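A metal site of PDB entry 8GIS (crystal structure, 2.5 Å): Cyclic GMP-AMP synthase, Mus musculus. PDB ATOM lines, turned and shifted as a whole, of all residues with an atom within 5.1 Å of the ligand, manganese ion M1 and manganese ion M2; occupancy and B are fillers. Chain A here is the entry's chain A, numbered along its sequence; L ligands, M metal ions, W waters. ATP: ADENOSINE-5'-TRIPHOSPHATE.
O2' of the ligand lies within hydrogen-bond range of OE1 of Glu 228 (2.4 Å).
The side-chain hydroxyl (OG) of Ser 225 lies within hydrogen-bond range of an oxygen (O2') of the ligand (2.7 Å).
The backbone NH (N) of Ser 56 lies close to an oxygen (O2B) of the ligand, 2.7 Å away.
OG of Ser 56 is in hydrogen-bond range of O2G of the ligand (2.7 Å).
The side-chain amino group (NZ) of Lys 259 lies within salt-bridge range of an oxygen (O2G) of the ligand (2.8 Å).
O1G of the ligand lies within hydrogen-bond range of OG of Ser 277.
NZ of Lys 281 lies within hydrogen-bond range of O3' of the ligand, 3.1 Å away.
A nitrogen (N3) of the ligand is in hydrogen-bond range of the guanidinium group of Arg 221, 3.1 Å away.
N of Asp 164 is in hydrogen-bond range of O of Phe 69, 2.9 Å away.
The side-chain carboxylate (OE1) of Glu 228 lies within salt-bridge range of the side-chain amino group (NZ) of Lys 281 (2.7 Å).
The side-chain carboxylate (OE2) of Glu 228 lies within hydrogen-bond range of the side-chain hydroxyl (OH) of Tyr 278 (2.6 Å).
The backbone carbonyl oxygen (O) of Ser 56 lies within hydrogen-bond range of the backbone NH (N) of Lys 62 (3.3 Å).
The backbone NH (N) of Val 61 is in hydrogen-bond range of the backbone carbonyl oxygen (O) of Ser 56, at 2.9 Å.
NZ of Lys 281 is in salt-bridge range of OE2 of Glu 59, at 2.7 Å.
N of Tyr 278 lies close to SG of Cys 276 (3.7 Å).
Gly 55 touches the ligand (CA to O2B, 3.2 Å).
Lys 62 touches the ligand (CD to O2G, 3.9 Å).
Tyr 278 touches the ligand.
12 residues have an atom within 4 Å of the ligand: Gly 55, Ser 56, Lys 62, Glu 68, Asp 70, Arg 221, Ser 225, Glu 228, Lys 259, Ser 277, Tyr 278 and Lys 281.
Within 4 Å of manganese ion M1: Glu 68, Asp 70 and Asp 164.
Ser 56 touches manganese ion M2 (OG to MN, 3.9 Å).
Within 4 Å of manganese ion M2: Ser 56, Glu 68 and Asp 70.
OE2 of Glu 68 binds manganese ion M1.
OD1 of Asp 70 is bound to manganese ion M1, 2.2 Å away.
Manganese ion M1 is bound by the side-chain carboxylate (OD2) of Asp 164 (2.3 Å).
O2A of the ligand is bound to manganese ion M1 (2.3 Å).
Manganese ion M1 has four donor atoms within binding distance.
Manganese ion M2 is bound by the side-chain carboxylate of Glu 68, the side-chain carboxylate of Asp 70, an oxygen (O3G) of the ligand, an oxygen (O2A) of the ligand, water W1 and an oxygen (O2B) of the ligand.
Water W1 lies within hydrogen-bond range of the side-chain hydroxyl (OG) of Ser 56 (2.7 Å), the backbone carbonyl oxygen (O) of Glu 68 (2.8 Å) and the backbone NH (N) of Tyr 57 (3.4 Å).
Water W2 lies within hydrogen-bond range of an oxygen (O2G) of the ligand (2.5 Å) and the side-chain amino group of Lys 62 (2.9 Å).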
ATOM      1  N   GLY A  55      11.111  22.265  -8.124  1.00  0.00           N
ATOM      2  CA  GLY A  55      10.464  23.535  -7.841  1.00  0.00           C
ATOM      3  C   GLY A  55       9.119  23.667  -8.536  1.00  0.00           C
ATOM      4  O   GLY A  55       8.623  22.759  -9.201  1.00  0.00           O
ATOM      5  N   SER A  56       8.537  24.859  -8.374  1.00  0.00           N
ATOM      6  CA  SER A  56       7.111  25.019  -8.625  1.00  0.00           C
ATOM      7  C   SER A  56       6.769  24.736 -10.082  1.00  0.00           C
ATOM      8  O   SER A  56       5.702  24.175 -10.363  1.00  0.00           O
ATOM      9  CB  SER A  56       6.637  26.424  -8.239  1.00  0.00           C
ATOM     10  OG  SER A  56       7.317  27.463  -8.935  1.00  0.00           O
ATOM     11  N   TYR A  57       7.656  25.105 -11.008  1.00  0.00           N
ATOM     12  CA  TYR A  57       7.300  24.957 -12.410  1.00  0.00           C
ATOM     13  C   TYR A  57       7.120  23.494 -12.793  1.00  0.00           C
ATOM     14  O   TYR A  57       6.251  23.163 -13.599  1.00  0.00           O
ATOM     15  CB  TYR A  57       8.355  25.621 -13.291  1.00  0.00           C
ATOM     16  CG  TYR A  57       8.152  25.341 -14.762  1.00  0.00           C
ATOM     17  CD1 TYR A  57       7.232  26.093 -15.512  1.00  0.00           C
ATOM     18  CD2 TYR A  57       8.837  24.311 -15.405  1.00  0.00           C
ATOM     19  CE1 TYR A  57       7.018  25.825 -16.861  1.00  0.00           C
ATOM     20  CE2 TYR A  57       8.632  24.042 -16.758  1.00  0.00           C
ATOM     21  CZ  TYR A  57       7.720  24.820 -17.476  1.00  0.00           C
ATOM     22  OH  TYR A  57       7.514  24.559 -18.808  1.00  0.00           O
ATOM     23  N   GLU A  59       6.409  21.150 -10.509  1.00  0.00           N
ATOM     24  CA  GLU A  59       5.294  20.634  -9.738  1.00  0.00           C
ATOM     25  C   GLU A  59       3.953  21.150 -10.269  1.00  0.00           C
ATOM     26  O   GLU A  59       2.906  20.737  -9.775  1.00  0.00           O
ATOM     27  CB  GLU A  59       5.465  20.999  -8.252  1.00  0.00           C
ATOM     28  CG  GLU A  59       6.767  20.437  -7.607  1.00  0.00           C
ATOM     29  CD  GLU A  59       7.239  21.277  -6.398  1.00  0.00           C
ATOM     30  OE1 GLU A  59       6.910  22.490  -6.329  1.00  0.00           O
ATOM     31  OE2 GLU A  59       7.968  20.738  -5.524  1.00  0.00           O
ATOM     32  N   VAL A  61       2.857  24.210  -9.911  1.00  0.00           N
ATOM     33  CA  VAL A  61       2.257  25.215  -9.032  1.00  0.00           C
ATOM     34  C   VAL A  61       2.886  26.601  -9.215  1.00  0.00           C
ATOM     35  O   VAL A  61       2.663  27.492  -8.385  1.00  0.00           O
ATOM     36  CB  VAL A  61       2.277  24.761  -7.556  1.00  0.00           C
ATOM     37  CG1 VAL A  61       1.307  23.600  -7.370  1.00  0.00           C
ATOM     38  CG2 VAL A  61       3.668  24.358  -7.115  1.00  0.00           C
ATOM     39  N   LYS A  62       3.686  26.786 -10.279  1.00  0.00           N
ATOM     40  CA  LYS A  62       4.171  28.104 -10.660  1.00  0.00           C
ATOM     41  C   LYS A  62       3.006  29.004 -11.046  1.00  0.00           C
ATOM     42  O   LYS A  62       2.182  28.627 -11.879  1.00  0.00           O
ATOM     43  CB  LYS A  62       5.126  27.964 -11.852  1.00  0.00           C
ATOM     44  CG  LYS A  62       5.778  29.270 -12.303  1.00  0.00           C
ATOM     45  CD  LYS A  62       6.872  29.635 -11.326  1.00  0.00           C
ATOM     46  CE  LYS A  62       7.435  31.001 -11.600  1.00  0.00           C
ATOM     47  NZ  LYS A  62       6.566  32.095 -11.107  1.00  0.00           N
ATOM     48  N   GLU A  68      10.543  31.686 -13.566  1.00  0.00           N
ATOM     49  CA  GLU A  68      11.544  31.207 -12.605  1.00  0.00           C
ATOM     50  C   GLU A  68      11.550  29.686 -12.608  1.00  0.00           C
ATOM     51  O   GLU A  68      10.499  29.071 -12.385  1.00  0.00           O
ATOM     52  CB  GLU A  68      11.283  31.745 -11.204  1.00  0.00           C
ATOM     53  CG  GLU A  68      12.535  31.816 -10.334  1.00  0.00           C
ATOM     54  CD  GLU A  68      12.720  30.557  -9.478  1.00  0.00           C
ATOM     55  OE1 GLU A  68      11.859  29.678  -9.563  1.00  0.00           O
ATOM     56  OE2 GLU A  68      13.703  30.441  -8.734  1.00  0.00           O
ATOM     57  N   PHE A  69      12.740  29.109 -12.834  1.00  0.00           N
ATOM     58  CA  PHE A  69      12.959  27.675 -13.001  1.00  0.00           C
ATOM     59  C   PHE A  69      14.058  27.240 -12.038  1.00  0.00           C
ATOM     60  O   PHE A  69      15.043  27.958 -11.872  1.00  0.00           O
ATOM     61  CB  PHE A  69      13.400  27.310 -14.454  1.00  0.00           C
ATOM     62  CG  PHE A  69      12.365  27.631 -15.495  1.00  0.00           C
ATOM     63  CD1 PHE A  69      12.117  28.943 -15.879  1.00  0.00           C
ATOM     64  CD2 PHE A  69      11.618  26.620 -16.078  1.00  0.00           C
ATOM     65  CE1 PHE A  69      11.144  29.244 -16.846  1.00  0.00           C
ATOM     66  CE2 PHE A  69      10.639  26.917 -17.029  1.00  0.00           C
ATOM     67  CZ  PHE A  69      10.404  28.231 -17.408  1.00  0.00           C
ATOM     68  N   ASP A  70      13.881  26.089 -11.408  1.00  0.00           N
ATOM     69  CA  ASP A  70      14.892  25.562 -10.503  1.00  0.00           C
ATOM     70  C   ASP A  70      15.391  24.229 -11.021  1.00  0.00           C
ATOM     71  O   ASP A  70      14.593  23.357 -11.374  1.00  0.00           O
ATOM     72  CB  ASP A  70      14.331  25.390  -9.096  1.00  0.00           C
ATOM     73  CG  ASP A  70      13.725  26.663  -8.592  1.00  0.00           C
ATOM     74  OD1 ASP A  70      14.486  27.579  -8.216  1.00  0.00           O
ATOM     75  OD2 ASP A  70      12.481  26.752  -8.590  1.00  0.00           O
ATOM     76  N   ASP A 164      17.654  29.027 -11.415  1.00  0.00           N
ATOM     77  CA  ASP A 164      18.540  28.668 -10.314  1.00  0.00           C
ATOM     78  C   ASP A 164      19.205  27.330 -10.624  1.00  0.00           C
ATOM     79  O   ASP A 164      18.523  26.295 -10.708  1.00  0.00           O
ATOM     80  CB  ASP A 164      17.753  28.592  -9.015  1.00  0.00           C
ATOM     81  CG  ASP A 164      17.428  29.967  -8.474  1.00  0.00           C
ATOM     82  OD1 ASP A 164      18.211  30.910  -8.755  1.00  0.00           O
ATOM     83  OD2 ASP A 164      16.403  30.099  -7.777  1.00  0.00           O
ATOM     84  N   ARG A 221      23.515  21.781   3.596  1.00  0.00           N
ATOM     85  CA  ARG A 221      22.119  21.749   4.025  1.00  0.00           C
ATOM     86  C   ARG A 221      21.393  20.641   3.280  1.00  0.00           C
ATOM     87  O   ARG A 221      21.578  20.466   2.069  1.00  0.00           O
ATOM     88  CB  ARG A 221      21.443  23.126   3.775  1.00  0.00           C
ATOM     89  CG  ARG A 221      20.040  23.321   4.385  1.00  0.00           C
ATOM     90  CD  ARG A 221      19.218  24.373   3.642  1.00  0.00           C
ATOM     91  NE  ARG A 221      18.352  23.720   2.664  1.00  0.00           N
ATOM     92  CZ  ARG A 221      18.135  24.165   1.429  1.00  0.00           C
ATOM     93  NH1 ARG A 221      18.599  25.337   1.017  1.00  0.00           N
ATOM     94  NH2 ARG A 221      17.446  23.396   0.583  1.00  0.00           N
ATOM     95  N   LEU A 222      20.569  19.869   4.003  1.00  0.00           N
ATOM     96  CA  LEU A 222      19.768  18.805   3.399  1.00  0.00           C
ATOM     97  C   LEU A 222      18.718  19.363   2.440  1.00  0.00           C
ATOM     98  O   LEU A 222      18.076  20.381   2.726  1.00  0.00           O
ATOM     99  CB  LEU A 222      19.067  17.970   4.465  1.00  0.00           C
ATOM    100  CG  LEU A 222      19.886  16.895   5.159  1.00  0.00           C
ATOM    101  CD1 LEU A 222      19.133  16.341   6.355  1.00  0.00           C
ATOM    102  CD2 LEU A 222      20.198  15.788   4.150  1.00  0.00           C
ATOM    103  N   PHE A 224      15.334  18.079  -0.071  1.00  0.00           N
ATOM    104  CA  PHE A 224      14.335  17.071  -0.390  1.00  0.00           C
ATOM    105  C   PHE A 224      13.450  17.548  -1.520  1.00  0.00           C
ATOM    106  O   PHE A 224      12.274  17.171  -1.573  1.00  0.00           O
ATOM    107  CB  PHE A 224      13.488  16.714   0.826  1.00  0.00           C
ATOM    108  CG  PHE A 224      14.280  16.068   1.923  1.00  0.00           C
ATOM    109  CD1 PHE A 224      14.682  14.757   1.788  1.00  0.00           C
ATOM    110  CD2 PHE A 224      14.682  16.793   3.026  1.00  0.00           C
ATOM    111  CE1 PHE A 224      15.459  14.159   2.750  1.00  0.00           C
ATOM    112  CE2 PHE A 224      15.450  16.188   4.020  1.00  0.00           C
ATOM    113  CZ  PHE A 224      15.838  14.885   3.876  1.00  0.00           C
ATOM    114  N   SER A 225      13.995  18.389  -2.409  1.00  0.00           N
ATOM    115  CA  SER A 225      13.198  18.894  -3.526  1.00  0.00           C
ATOM    116  C   SER A 225      12.607  17.758  -4.329  1.00  0.00           C
ATOM    117  O   SER A 225      11.467  17.854  -4.786  1.00  0.00           O
ATOM    118  CB  SER A 225      14.035  19.780  -4.430  1.00  0.00           C
ATOM    119  OG  SER A 225      14.289  21.002  -3.782  1.00  0.00           O
ATOM    120  N   GLU A 228       9.587  16.337  -2.475  1.00  0.00           N
ATOM    121  CA  GLU A 228       8.484  17.287  -2.586  1.00  0.00           C
ATOM    122  C   GLU A 228       7.854  17.236  -3.974  1.00  0.00           C
ATOM    123  O   GLU A 228       6.636  17.387  -4.099  1.00  0.00           O
ATOM    124  CB  GLU A 228       8.986  18.693  -2.249  1.00  0.00           C
ATOM    125  CG  GLU A 228       9.565  18.805  -0.826  1.00  0.00           C
ATOM    126  CD  GLU A 228      10.487  20.002  -0.649  1.00  0.00           C
ATOM    127  OE1 GLU A 228      10.545  20.864  -1.549  1.00  0.00           O
ATOM    128  OE2 GLU A 228      11.145  20.113   0.416  1.00  0.00           O
ATOM    129  N   LYS A 259       0.562  30.929  -2.191  1.00  0.00           N
ATOM    130  CA  LYS A 259       1.786  31.455  -2.793  1.00  0.00           C
ATOM    131  C   LYS A 259       1.584  32.894  -3.259  1.00  0.00           C
ATOM    132  O   LYS A 259       2.461  33.753  -3.051  1.00  0.00           O
ATOM    133  CB  LYS A 259       2.205  30.604  -3.987  1.00  0.00           C
ATOM    134  CG  LYS A 259       2.931  29.317  -3.610  1.00  0.00           C
ATOM    135  CD  LYS A 259       2.920  28.343  -4.792  1.00  0.00           C
ATOM    136  CE  LYS A 259       3.694  28.944  -5.935  1.00  0.00           C
ATOM    137  NZ  LYS A 259       5.162  28.779  -5.715  1.00  0.00           N
ATOM    138  N   GLU A 263       3.466  36.270  -2.231  1.00  0.00           N
ATOM    139  CA  GLU A 263       4.159  36.979  -3.307  1.00  0.00           C
ATOM    140  C   GLU A 263       3.686  38.435  -3.407  1.00  0.00           C
ATOM    141  O   GLU A 263       4.496  39.369  -3.467  1.00  0.00           O
ATOM    142  CB  GLU A 263       3.913  36.221  -4.623  1.00  0.00           C
ATOM    143  CG  GLU A 263       5.086  36.057  -5.552  1.00  0.00           C
ATOM    144  CD  GLU A 263       4.879  34.928  -6.572  1.00  0.00           C
ATOM    145  OE1 GLU A 263       4.908  35.237  -7.788  1.00  0.00           O
ATOM    146  OE2 GLU A 263       4.743  33.739  -6.214  1.00  0.00           O
ATOM    147  N   CYS A 276       9.529  33.316   2.651  1.00  0.00           N
ATOM    148  CA  CYS A 276       9.691  32.825   1.304  1.00  0.00           C
ATOM    149  C   CYS A 276       8.623  31.772   1.054  1.00  0.00           C
ATOM    150  O   CYS A 276       8.037  31.228   1.988  1.00  0.00           O
ATOM    151  CB  CYS A 276      11.092  32.246   1.078  1.00  0.00           C
ATOM    152  SG  CYS A 276      11.421  30.763   2.070  1.00  0.00           S
ATOM    153  N   SER A 277       8.408  31.468  -0.229  1.00  0.00           N
ATOM    154  CA  SER A 277       7.342  30.533  -0.558  1.00  0.00           C
ATOM    155  C   SER A 277       7.573  29.130   0.010  1.00  0.00           C
ATOM    156  O   SER A 277       6.609  28.364   0.122  1.00  0.00           O
ATOM    157  CB  SER A 277       7.158  30.486  -2.072  1.00  0.00           C
ATOM    158  OG  SER A 277       8.338  30.054  -2.701  1.00  0.00           O
ATOM    159  N   TYR A 278       8.795  28.789   0.414  1.00  0.00           N
ATOM    160  CA  TYR A 278       8.975  27.483   1.050  1.00  0.00           C
ATOM    161  C   TYR A 278       8.189  27.398   2.354  1.00  0.00           C
ATOM    162  O   TYR A 278       7.796  26.312   2.787  1.00  0.00           O
ATOM    163  CB  TYR A 278      10.460  27.179   1.324  1.00  0.00           C
ATOM    164  CG  TYR A 278      10.699  25.722   1.681  1.00  0.00           C
ATOM    165  CD1 TYR A 278      10.509  24.718   0.742  1.00  0.00           C
ATOM    166  CD2 TYR A 278      11.072  25.323   2.972  1.00  0.00           C
ATOM    167  CE1 TYR A 278      10.705  23.379   1.043  1.00  0.00           C
ATOM    168  CE2 TYR A 278      11.272  23.979   3.285  1.00  0.00           C
ATOM    169  CZ  TYR A 278      11.073  23.022   2.304  1.00  0.00           C
ATOM    170  OH  TYR A 278      11.262  21.666   2.544  1.00  0.00           O
ATOM    171  N   LYS A 281       4.796  26.361   1.403  1.00  0.00           N
ATOM    172  CA  LYS A 281       4.833  24.980   0.918  1.00  0.00           C
ATOM    173  C   LYS A 281       4.913  24.010   2.086  1.00  0.00           C
ATOM    174  O   LYS A 281       4.211  22.980   2.108  1.00  0.00           O
ATOM    175  CB  LYS A 281       6.029  24.780  -0.020  1.00  0.00           C
ATOM    176  CG  LYS A 281       6.020  23.488  -0.838  1.00  0.00           C
ATOM    177  CD  LYS A 281       7.224  23.442  -1.777  1.00  0.00           C
ATOM    178  CE  LYS A 281       7.229  22.170  -2.623  1.00  0.00           C
ATOM    179  NZ  LYS A 281       8.596  21.883  -3.197  1.00  0.00           N
ATOM    180  N   HIS A 324      10.058  22.039   9.850  1.00  0.00           N
ATOM    181  CA  HIS A 324      10.455  21.424   8.595  1.00  0.00           C
ATOM    182  C   HIS A 324       9.748  20.084   8.421  1.00  0.00           C
ATOM    183  O   HIS A 324       9.681  19.278   9.347  1.00  0.00           O
ATOM    184  CB  HIS A 324      11.976  21.233   8.591  1.00  0.00           C
ATOM    185  CG  HIS A 324      12.554  21.019   7.229  1.00  0.00           C
ATOM    186  ND1 HIS A 324      12.337  19.871   6.503  1.00  0.00           N
ATOM    187  CD2 HIS A 324      13.343  21.806   6.468  1.00  0.00           C
ATOM    188  CE1 HIS A 324      12.964  19.958   5.343  1.00  0.00           C
ATOM    189  NE2 HIS A 324      13.586  21.123   5.301  1.00  0.00           N
HETATM  190  PG  ATP L   1       8.344  29.668  -6.498  1.00  0.00           P
HETATM  191  O1G ATP L   1       8.384  30.717  -5.440  1.00  0.00           O
HETATM  192  O2G ATP L   1       7.133  29.684  -7.466  1.00  0.00           O
HETATM  193  O3G ATP L   1       9.573  29.671  -7.351  1.00  0.00           O
HETATM  194  PB  ATP L   1       9.417  27.056  -5.503  1.00  0.00           P
HETATM  195  O1B ATP L   1       8.912  25.993  -4.594  1.00  0.00           O
HETATM  196  O2B ATP L   1       9.981  26.548  -6.833  1.00  0.00           O
HETATM  197  O3B ATP L   1       8.358  28.200  -5.836  1.00  0.00           O
HETATM  198  PA  ATP L   1      12.069  28.238  -4.850  1.00  0.00           P
HETATM  199  O1A ATP L   1      12.469  29.286  -3.882  1.00  0.00           O
HETATM  200  O2A ATP L   1      12.312  28.597  -6.287  1.00  0.00           O
HETATM  201  O3A ATP L   1      10.510  27.908  -4.710  1.00  0.00           O
HETATM  202  O5' ATP L   1      12.866  26.956  -4.390  1.00  0.00           O
HETATM  203  C5' ATP L   1      13.036  25.819  -5.252  1.00  0.00           C
HETATM  204  C4' ATP L   1      12.997  24.597  -4.368  1.00  0.00           C
HETATM  205  O4' ATP L   1      14.119  24.608  -3.464  1.00  0.00           O
HETATM  206  C3' ATP L   1      11.775  24.511  -3.457  1.00  0.00           C
HETATM  207  O3' ATP L   1      10.657  23.943  -4.134  1.00  0.00           O
HETATM  208  C2' ATP L   1      12.285  23.626  -2.309  1.00  0.00           C
HETATM  209  O2' ATP L   1      12.251  22.239  -2.596  1.00  0.00           O
HETATM  210  C1' ATP L   1      13.736  24.084  -2.195  1.00  0.00           C
HETATM  211  N9  ATP L   1      13.929  25.121  -1.187  1.00  0.00           N
HETATM  212  C8  ATP L   1      13.811  26.481  -1.344  1.00  0.00           C
HETATM  213  N7  ATP L   1      14.025  27.171  -0.249  1.00  0.00           N
HETATM  214  C5  ATP L   1      14.275  26.187   0.703  1.00  0.00           C
HETATM  215  C6  ATP L   1      14.565  26.271   2.084  1.00  0.00           C
HETATM  216  N6  ATP L   1      14.671  27.418   2.759  1.00  0.00           N
HETATM  217  N1  ATP L   1      14.771  25.097   2.743  1.00  0.00           N
HETATM  218  C2  ATP L   1      14.678  23.952   2.072  1.00  0.00           C
HETATM  219  N3  ATP L   1      14.405  23.765   0.779  1.00  0.00           N
HETATM  220  C4  ATP L   1      14.207  24.928   0.144  1.00  0.00           C
HETATM  221 MN    MN M   1      14.401  29.390  -6.964  1.00  0.00          MN
HETATM  222 MN    MN M   2      11.049  28.306  -8.159  1.00  0.00          MN
HETATM  223  O   HOH W   1       9.813  27.608 -10.054  1.00  0.00           O
HETATM  224  O   HOH W   2       5.399  31.109  -8.657  1.00  0.00           O
